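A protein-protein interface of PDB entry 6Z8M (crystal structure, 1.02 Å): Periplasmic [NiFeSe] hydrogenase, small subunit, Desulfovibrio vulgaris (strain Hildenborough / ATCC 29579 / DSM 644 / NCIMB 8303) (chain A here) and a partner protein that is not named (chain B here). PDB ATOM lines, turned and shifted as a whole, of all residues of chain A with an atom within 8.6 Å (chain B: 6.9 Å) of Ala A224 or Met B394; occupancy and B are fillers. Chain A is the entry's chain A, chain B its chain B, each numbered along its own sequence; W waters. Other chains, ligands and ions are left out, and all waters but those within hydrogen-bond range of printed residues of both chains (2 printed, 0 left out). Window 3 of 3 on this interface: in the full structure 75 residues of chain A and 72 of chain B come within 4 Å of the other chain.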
ATOM      1  N   VAL A 221     -28.991 -14.182 -15.543  1.00  0.00           N
ATOM      2  CA  VAL A 221     -28.722 -13.623 -14.221  1.00  0.00           C
ATOM      3  C   VAL A 221     -27.625 -14.473 -13.586  1.00  0.00           C
ATOM      4  O   VAL A 221     -27.882 -15.579 -13.110  1.00  0.00           O
ATOM      5  CB  VAL A 221     -29.986 -13.587 -13.362  1.00  0.00           C
ATOM      6  CG1 VAL A 221     -29.662 -13.051 -11.975  1.00  0.00           C
ATOM      7  CG2 VAL A 221     -31.067 -12.707 -14.030  1.00  0.00           C
ATOM      8  N   MET A 222     -26.401 -13.944 -13.586  1.00  0.00           N
ATOM      9  CA  MET A 222     -25.207 -14.680 -13.195  1.00  0.00           C
ATOM     10  C   MET A 222     -24.596 -14.055 -11.954  1.00  0.00           C
ATOM     11  O   MET A 222     -24.369 -12.841 -11.911  1.00  0.00           O
ATOM     12  CB  MET A 222     -24.169 -14.615 -14.310  1.00  0.00           C
ATOM     13  CG  MET A 222     -24.631 -15.209 -15.590  1.00  0.00           C
ATOM     14  SD  MET A 222     -24.819 -16.984 -15.393  1.00  0.00           S
ATOM     15  CE  MET A 222     -25.508 -17.362 -17.016  1.00  0.00           C
ATOM     16  N   SER A 223     -24.277 -14.892 -10.976  1.00  0.00           N
ATOM     17  CA  SER A 223     -23.565 -14.403  -9.804  1.00  0.00           C
ATOM     18  C   SER A 223     -22.161 -13.949 -10.181  1.00  0.00           C
ATOM     19  O   SER A 223     -21.468 -14.604 -10.964  1.00  0.00           O
ATOM     20  CB  SER A 223     -23.504 -15.503  -8.752  1.00  0.00           C
ATOM     21  OG  SER A 223     -24.819 -15.780  -8.315  1.00  0.00           O
ATOM     22  N   ALA A 224     -21.739 -12.819  -9.614  1.00  0.00           N
ATOM     23  CA  ALA A 224     -20.397 -12.298  -9.819  1.00  0.00           C
ATOM     24  C   ALA A 224     -19.459 -12.619  -8.670  1.00  0.00           C
ATOM     25  O   ALA A 224     -18.241 -12.458  -8.814  1.00  0.00           O
ATOM     26  CB  ALA A 224     -20.435 -10.780  -9.999  1.00  0.00           C
ATOM     27  N   THR A 225     -19.999 -13.052  -7.541  1.00  0.00           N
ATOM     28  CA  THR A 225     -19.219 -13.534  -6.421  1.00  0.00           C
ATOM     29  C   THR A 225     -19.811 -14.858  -5.981  1.00  0.00           C
ATOM     30  O   THR A 225     -21.020 -15.077  -6.088  1.00  0.00           O
ATOM     31  CB  THR A 225     -19.214 -12.557  -5.250  1.00  0.00           C
ATOM     32  OG1 THR A 225     -18.575 -13.195  -4.139  1.00  0.00           O
ATOM     33  CG2 THR A 225     -20.623 -12.126  -4.847  1.00  0.00           C
ATOM     34  N   PHE A 226     -18.948 -15.741  -5.479  1.00  0.00           N
ATOM     35  CA  PHE A 226     -19.418 -17.048  -5.055  1.00  0.00           C
ATOM     36  C   PHE A 226     -20.528 -16.949  -4.026  1.00  0.00           C
ATOM     37  O   PHE A 226     -21.408 -17.812  -3.998  1.00  0.00           O
ATOM     38  CB  PHE A 226     -18.281 -17.862  -4.441  1.00  0.00           C
ATOM     39  CG  PHE A 226     -17.238 -18.311  -5.431  1.00  0.00           C
ATOM     40  CD1 PHE A 226     -17.515 -19.300  -6.356  1.00  0.00           C
ATOM     41  CD2 PHE A 226     -15.971 -17.755  -5.419  1.00  0.00           C
ATOM     42  CE1 PHE A 226     -16.538 -19.717  -7.254  1.00  0.00           C
ATOM     43  CE2 PHE A 226     -15.009 -18.161  -6.309  1.00  0.00           C
ATOM     44  CZ  PHE A 226     -15.287 -19.135  -7.224  1.00  0.00           C
ATOM     45  N   THR A 227     -20.501 -15.935  -3.169  1.00  0.00           N
ATOM     46  CA  THR A 227     -21.447 -15.889  -2.063  1.00  0.00           C
ATOM     47  C   THR A 227     -22.824 -15.371  -2.460  1.00  0.00           C
ATOM     48  O   THR A 227     -23.733 -15.404  -1.628  1.00  0.00           O
ATOM     49  CB  THR A 227     -20.862 -15.083  -0.903  1.00  0.00           C
ATOM     50  OG1 THR A 227     -20.435 -13.811  -1.389  1.00  0.00           O
ATOM     51  CG2 THR A 227     -19.675 -15.829  -0.279  1.00  0.00           C
ATOM     52  N   ASP A 228     -23.010 -14.919  -3.700  1.00  0.00           N
ATOM     53  CA  ASP A 228     -24.340 -14.595  -4.215  1.00  0.00           C
ATOM     54  C   ASP A 228     -25.015 -15.896  -4.634  1.00  0.00           C
ATOM     55  O   ASP A 228     -24.668 -16.487  -5.660  1.00  0.00           O
ATOM     56  CB  ASP A 228     -24.210 -13.624  -5.385  1.00  0.00           C
ATOM     57  CG  ASP A 228     -25.529 -13.340  -6.076  1.00  0.00           C
ATOM     58  OD1 ASP A 228     -26.565 -13.950  -5.732  1.00  0.00           O
ATOM     59  OD2 ASP A 228     -25.511 -12.485  -6.983  1.00  0.00           O
ATOM     60  N   LYS A 229     -25.967 -16.353  -3.831  1.00  0.00           N
ATOM     61  CA  LYS A 229     -26.618 -17.630  -4.079  1.00  0.00           C
ATOM     62  C   LYS A 229     -27.889 -17.501  -4.905  1.00  0.00           C
ATOM     63  O   LYS A 229     -28.562 -18.515  -5.140  1.00  0.00           O
ATOM     64  CB  LYS A 229     -26.909 -18.349  -2.756  1.00  0.00           C
ATOM     65  CG  LYS A 229     -25.665 -18.631  -1.908  1.00  0.00           C
ATOM     66  CD  LYS A 229     -24.514 -19.195  -2.729  1.00  0.00           C
ATOM     67  CE  LYS A 229     -23.422 -19.798  -1.885  1.00  0.00           C
ATOM     68  NZ  LYS A 229     -22.267 -20.180  -2.738  1.00  0.00           N
ATOM     69  N   VAL A 230     -28.225 -16.291  -5.356  1.00  0.00           N
ATOM     70  CA  VAL A 230     -29.421 -16.101  -6.173  1.00  0.00           C
ATOM     71  C   VAL A 230     -29.150 -16.420  -7.638  1.00  0.00           C
ATOM     72  O   VAL A 230     -29.972 -17.057  -8.306  1.00  0.00           O
ATOM     73  CB  VAL A 230     -29.953 -14.667  -6.002  1.00  0.00           C
ATOM     74  CG1 VAL A 230     -31.100 -14.405  -6.987  1.00  0.00           C
ATOM     75  CG2 VAL A 230     -30.402 -14.439  -4.569  1.00  0.00           C
ATOM     76  N   GLY A 231     -28.041 -15.949  -8.176  1.00  0.00           N
ATOM     77  CA  GLY A 231     -27.778 -16.113  -9.586  1.00  0.00           C
ATOM     78  C   GLY A 231     -27.258 -17.490  -9.953  1.00  0.00           C
ATOM     79  O   GLY A 231     -26.877 -18.313  -9.120  1.00  0.00           O
ATOM     80  N   CYS A 232     -27.245 -17.732 -11.259  1.00  0.00           N
ATOM     81  CA  CYS A 232     -26.606 -18.914 -11.805  1.00  0.00           C
ATOM     82  C   CYS A 232     -25.087 -18.796 -11.658  1.00  0.00           C
ATOM     83  O   CYS A 232     -24.522 -17.694 -11.653  1.00  0.00           O
ATOM     84  CB  CYS A 232     -27.025 -19.075 -13.265  1.00  0.00           C
ATOM     85  SG  CYS A 232     -26.050 -20.193 -14.284  1.00  0.00           S
ATOM     86  N   ARG A 233     -24.439 -19.953 -11.512  1.00  0.00           N
ATOM     87  CA  ARG A 233     -23.006 -20.065 -11.267  1.00  0.00           C
ATOM     88  C   ARG A 233     -22.179 -20.246 -12.543  1.00  0.00           C
ATOM     89  O   ARG A 233     -20.965 -20.474 -12.462  1.00  0.00           O
ATOM     90  CB  ARG A 233     -22.761 -21.233 -10.320  1.00  0.00           C
ATOM     91  CG  ARG A 233     -23.178 -21.011  -8.866  1.00  0.00           C
ATOM     92  CD  ARG A 233     -24.674 -20.912  -8.605  1.00  0.00           C
ATOM     93  NE  ARG A 233     -24.949 -21.270  -7.217  1.00  0.00           N
ATOM     94  CZ  ARG A 233     -25.957 -20.819  -6.474  1.00  0.00           C
ATOM     95  NH1 ARG A 233     -26.853 -19.963  -6.954  1.00  0.00           N
ATOM     96  NH2 ARG A 233     -26.070 -21.238  -5.221  1.00  0.00           N
ATOM     97  N   TYR A 234     -22.791 -20.105 -13.717  1.00  0.00           N
ATOM     98  CA  TYR A 234     -22.084 -20.388 -14.963  1.00  0.00           C
ATOM     99  C   TYR A 234     -20.837 -19.523 -15.130  1.00  0.00           C
ATOM    100  O   TYR A 234     -19.779 -20.015 -15.540  1.00  0.00           O
ATOM    101  CB  TYR A 234     -23.041 -20.161 -16.125  1.00  0.00           C
ATOM    102  CG  TYR A 234     -22.448 -20.435 -17.470  1.00  0.00           C
ATOM    103  CD1 TYR A 234     -22.308 -21.729 -17.934  1.00  0.00           C
ATOM    104  CD2 TYR A 234     -22.042 -19.396 -18.292  1.00  0.00           C
ATOM    105  CE1 TYR A 234     -21.779 -21.981 -19.176  1.00  0.00           C
ATOM    106  CE2 TYR A 234     -21.513 -19.641 -19.541  1.00  0.00           C
ATOM    107  CZ  TYR A 234     -21.374 -20.937 -19.971  1.00  0.00           C
ATOM    108  OH  TYR A 234     -20.861 -21.179 -21.221  1.00  0.00           O
ATOM    109  N   ASP A 235     -20.950 -18.214 -14.877  1.00  0.00           N
ATOM    110  CA  ASP A 235     -19.806 -17.338 -15.110  1.00  0.00           C
ATOM    111  C   ASP A 235     -18.693 -17.599 -14.111  1.00  0.00           C
ATOM    112  O   ASP A 235     -17.532 -17.299 -14.400  1.00  0.00           O
ATOM    113  CB  ASP A 235     -20.203 -15.868 -15.006  1.00  0.00           C
ATOM    114  CG  ASP A 235     -20.937 -15.352 -16.224  1.00  0.00           C
ATOM    115  OD1 ASP A 235     -21.024 -16.044 -17.260  1.00  0.00           O
ATOM    116  OD2 ASP A 235     -21.413 -14.204 -16.130  1.00  0.00           O
ATOM    117  N   LEU A 236     -19.025 -18.142 -12.944  1.00  0.00           N
ATOM    118  CA  LEU A 236     -18.042 -18.546 -11.949  1.00  0.00           C
ATOM    119  C   LEU A 236     -17.395 -19.886 -12.282  1.00  0.00           C
ATOM    120  O   LEU A 236     -16.514 -20.328 -11.538  1.00  0.00           O
ATOM    121  CB  LEU A 236     -18.702 -18.623 -10.573  1.00  0.00           C
ATOM    122  CG  LEU A 236     -19.219 -17.297 -10.003  1.00  0.00           C
ATOM    123  CD1 LEU A 236     -20.145 -17.577  -8.820  1.00  0.00           C
ATOM    124  CD2 LEU A 236     -18.074 -16.394  -9.585  1.00  0.00           C
ATOM    125  N   GLY A 237     -17.809 -20.547 -13.364  1.00  0.00           N
ATOM    126  CA  GLY A 237     -17.164 -21.762 -13.832  1.00  0.00           C
ATOM    127  C   GLY A 237     -17.997 -23.027 -13.774  1.00  0.00           C
ATOM    128  O   GLY A 237     -17.472 -24.107 -14.079  1.00  0.00           O
ATOM    129  N   TYR A 281     -12.779 -22.202 -12.693  1.00  0.00           N
ATOM    130  CA  TYR A 281     -13.430 -20.995 -12.213  1.00  0.00           C
ATOM    131  C   TYR A 281     -13.653 -19.970 -13.309  1.00  0.00           C
ATOM    132  O   TYR A 281     -13.817 -18.777 -13.029  1.00  0.00           O
ATOM    133  CB  TYR A 281     -12.682 -20.443 -11.010  1.00  0.00           C
ATOM    134  CG  TYR A 281     -12.735 -21.429  -9.871  1.00  0.00           C
ATOM    135  CD1 TYR A 281     -13.941 -21.728  -9.254  1.00  0.00           C
ATOM    136  CD2 TYR A 281     -11.608 -22.090  -9.441  1.00  0.00           C
ATOM    137  CE1 TYR A 281     -14.014 -22.635  -8.217  1.00  0.00           C
ATOM    138  CE2 TYR A 281     -11.663 -22.996  -8.399  1.00  0.00           C
ATOM    139  CZ  TYR A 281     -12.870 -23.271  -7.793  1.00  0.00           C
ATOM    140  OH  TYR A 281     -12.902 -24.176  -6.759  1.00  0.00           O
ATOM    141  N   ARG B  54      -5.972 -20.796  -9.799  1.00  0.00           N
ATOM    142  CA  ARG B  54      -7.150 -21.066  -8.985  1.00  0.00           C
ATOM    143  C   ARG B  54      -7.549 -22.525  -9.032  1.00  0.00           C
ATOM    144  O   ARG B  54      -8.183 -23.015  -8.097  1.00  0.00           O
ATOM    145  CB  ARG B  54      -8.314 -20.202  -9.458  1.00  0.00           C
ATOM    146  CG  ARG B  54      -8.078 -18.718  -9.257  1.00  0.00           C
ATOM    147  CD  ARG B  54      -9.142 -17.888  -9.928  1.00  0.00           C
ATOM    148  NE  ARG B  54      -9.085 -18.053 -11.370  1.00  0.00           N
ATOM    149  CZ  ARG B  54      -9.870 -17.409 -12.220  1.00  0.00           C
ATOM    150  NH1 ARG B  54     -10.762 -16.538 -11.770  1.00  0.00           N
ATOM    151  NH2 ARG B  54      -9.755 -17.632 -13.521  1.00  0.00           N
ATOM    152  N   ALA B  85      -4.960 -11.489  -2.042  1.00  0.00           N
ATOM    153  CA  ALA B  85      -6.347 -11.554  -1.613  1.00  0.00           C
ATOM    154  C   ALA B  85      -6.423 -11.337  -0.112  1.00  0.00           C
ATOM    155  O   ALA B  85      -5.668 -11.945   0.655  1.00  0.00           O
ATOM    156  CB  ALA B  85      -6.952 -12.910  -1.974  1.00  0.00           C
ATOM    157  N   VAL B 179     -11.741 -21.209  -1.488  1.00  0.00           N
ATOM    158  CA  VAL B 179     -11.160 -20.667  -2.707  1.00  0.00           C
ATOM    159  C   VAL B 179     -10.209 -19.554  -2.304  1.00  0.00           C
ATOM    160  O   VAL B 179     -10.270 -19.034  -1.193  1.00  0.00           O
ATOM    161  CB  VAL B 179     -12.235 -20.090  -3.676  1.00  0.00           C
ATOM    162  CG1 VAL B 179     -13.069 -21.193  -4.299  1.00  0.00           C
ATOM    163  CG2 VAL B 179     -13.121 -19.046  -2.965  1.00  0.00           C
ATOM    164  N   VAL B 180      -9.351 -19.154  -3.241  1.00  0.00           N
ATOM    165  CA  VAL B 180      -8.627 -17.907  -3.044  1.00  0.00           C
ATOM    166  C   VAL B 180      -9.634 -16.820  -2.700  1.00  0.00           C
ATOM    167  O   VAL B 180     -10.691 -16.708  -3.334  1.00  0.00           O
ATOM    168  CB  VAL B 180      -7.777 -17.558  -4.280  1.00  0.00           C
ATOM    169  CG1 VAL B 180      -8.631 -17.237  -5.504  1.00  0.00           C
ATOM    170  CG2 VAL B 180      -6.837 -16.405  -3.948  1.00  0.00           C
ATOM    171  N   GLY B 181      -9.325 -16.027  -1.676  1.00  0.00           N
ATOM    172  CA  GLY B 181     -10.196 -14.943  -1.285  1.00  0.00           C
ATOM    173  C   GLY B 181     -11.185 -15.269  -0.183  1.00  0.00           C
ATOM    174  O   GLY B 181     -11.849 -14.345   0.312  1.00  0.00           O
ATOM    175  N   VAL B 392     -16.042 -13.907   1.216  1.00  0.00           N
ATOM    176  CA  VAL B 392     -15.130 -14.030   0.087  1.00  0.00           C
ATOM    177  C   VAL B 392     -14.911 -12.685  -0.589  1.00  0.00           C
ATOM    178  O   VAL B 392     -15.806 -11.836  -0.632  1.00  0.00           O
ATOM    179  CB  VAL B 392     -15.629 -15.094  -0.931  1.00  0.00           C
ATOM    180  CG1 VAL B 392     -16.607 -14.487  -1.959  1.00  0.00           C
ATOM    181  CG2 VAL B 392     -14.461 -15.776  -1.633  1.00  0.00           C
ATOM    182  N   VAL B 393     -13.711 -12.522  -1.144  1.00  0.00           N
ATOM    183  CA  VAL B 393     -13.423 -11.504  -2.145  1.00  0.00           C
ATOM    184  C   VAL B 393     -13.103 -12.228  -3.448  1.00  0.00           C
ATOM    185  O   VAL B 393     -12.775 -13.415  -3.458  1.00  0.00           O
ATOM    186  CB  VAL B 393     -12.282 -10.557  -1.714  1.00  0.00           C
ATOM    187  CG1 VAL B 393     -12.704  -9.730  -0.506  1.00  0.00           C
ATOM    188  CG2 VAL B 393     -10.997 -11.328  -1.443  1.00  0.00           C
ATOM    189  N   MET B 394     -13.160 -11.487  -4.561  1.00  0.00           N
ATOM    190  CA  MET B 394     -12.999 -12.034  -5.911  1.00  0.00           C
ATOM    191  C   MET B 394     -11.784 -11.383  -6.575  1.00  0.00           C
ATOM    192  O   MET B 394     -11.922 -10.437  -7.354  1.00  0.00           O
ATOM    193  CB  MET B 394     -14.269 -11.816  -6.740  1.00  0.00           C
ATOM    194  CG  MET B 394     -15.527 -12.467  -6.146  1.00  0.00           C
ATOM    195  SD  MET B 394     -15.463 -14.277  -6.036  1.00  0.00           S
ATOM    196  CE  MET B 394     -15.247 -14.741  -7.743  1.00  0.00           C
ATOM    197  N   PRO B 395     -10.578 -11.876  -6.305  1.00  0.00           N
ATOM    198  CA  PRO B 395      -9.373 -11.217  -6.817  1.00  0.00           C
ATOM    199  C   PRO B 395      -9.010 -11.635  -8.229  1.00  0.00           C
ATOM    200  O   PRO B 395      -9.176 -12.787  -8.637  1.00  0.00           O
ATOM    201  CB  PRO B 395      -8.301 -11.706  -5.837  1.00  0.00           C
ATOM    202  CG  PRO B 395      -8.752 -13.091  -5.501  1.00  0.00           C
ATOM    203  CD  PRO B 395     -10.247 -12.988  -5.395  1.00  0.00           C
ATOM    204  N   ALA B 396      -8.476 -10.677  -8.979  1.00  0.00           N
ATOM    205  CA  ALA B 396      -7.989 -10.979 -10.314  1.00  0.00           C
ATOM    206  C   ALA B 396      -6.745 -11.859 -10.235  1.00  0.00           C
ATOM    207  O   ALA B 396      -5.943 -11.754  -9.307  1.00  0.00           O
ATOM    208  CB  ALA B 396      -7.647  -9.686 -11.051  1.00  0.00           C
HETATM  209  O   HOH W   1     -12.532 -15.806 -14.136  1.00  0.00           O
HETATM  210  O   HOH W   2     -18.115 -11.278  -2.194  1.00  0.00           O
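OG1 of Thr A225 sits at hydrogen-bond distance from OG1 of Thr A227, 3.4 Å away.
The backbone carbonyl oxygen of Phe A226 sits at hydrogen-bond distance from the side-chain amino group of Lys A229 (2.8 Å).
Among the printed residues, merely in contact across the chains: Thr A225 with Val B392, Tyr A281 with Arg B54, Phe A226 with Met B394, Thr A225 with Met B394, Thr A227 with Val B392, Leu A236 with Met B394, Ala A224 with Met B394, Tyr A281 with Val B179 and Phe A226 with Val B179.
Printed residues of chain B within 4 Å of Ala A224: Met B394 (3.8 Å).
No residue of chain A comes within 4 Å of Pro B395.
Of the printed residues of chain B, Thr A227 touches Val B392 (3.7 Å).
Of the printed residues of chain A, Val B179 touches Phe A226 and Tyr A281.
Printed residues of chain A within 4 Å of Arg B54: Tyr A281 (3.5 Å).
The nearest residue of chain A that does not touch Met B394 is Thr A227 (6.0 Å).
The nearest printed residue of chain B that does not touch Thr A225 is Val B393 (5.6 Å).
Hydrophobic or aromatic side chains of chain B within 4 Å of the printed part of chain A: Val B179, Val B392 and Met B394.
Hydrophobic or aromatic side chains of chain A within 4 Å of the printed part of chain B: Phe A226, Leu A236 and Tyr A281.
Along chain A the printed residues that touch a printed residue of chain B span positions 224 to 281.
Among the printed residues, 9 pairs touch across the chains.
Among the printed residues, no Asp or Glu carboxylate lies within 4 Å of a Lys or Arg side-chain nitrogen of the other chain.
Water W2 bridges OG1 of Thr A225 (2.8 Å) and O of Val B392 (2.8 Å).
Water W1 bridges NH1 of Arg B54 (3.0 Å) and O of Tyr A281 (3.4 Å).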
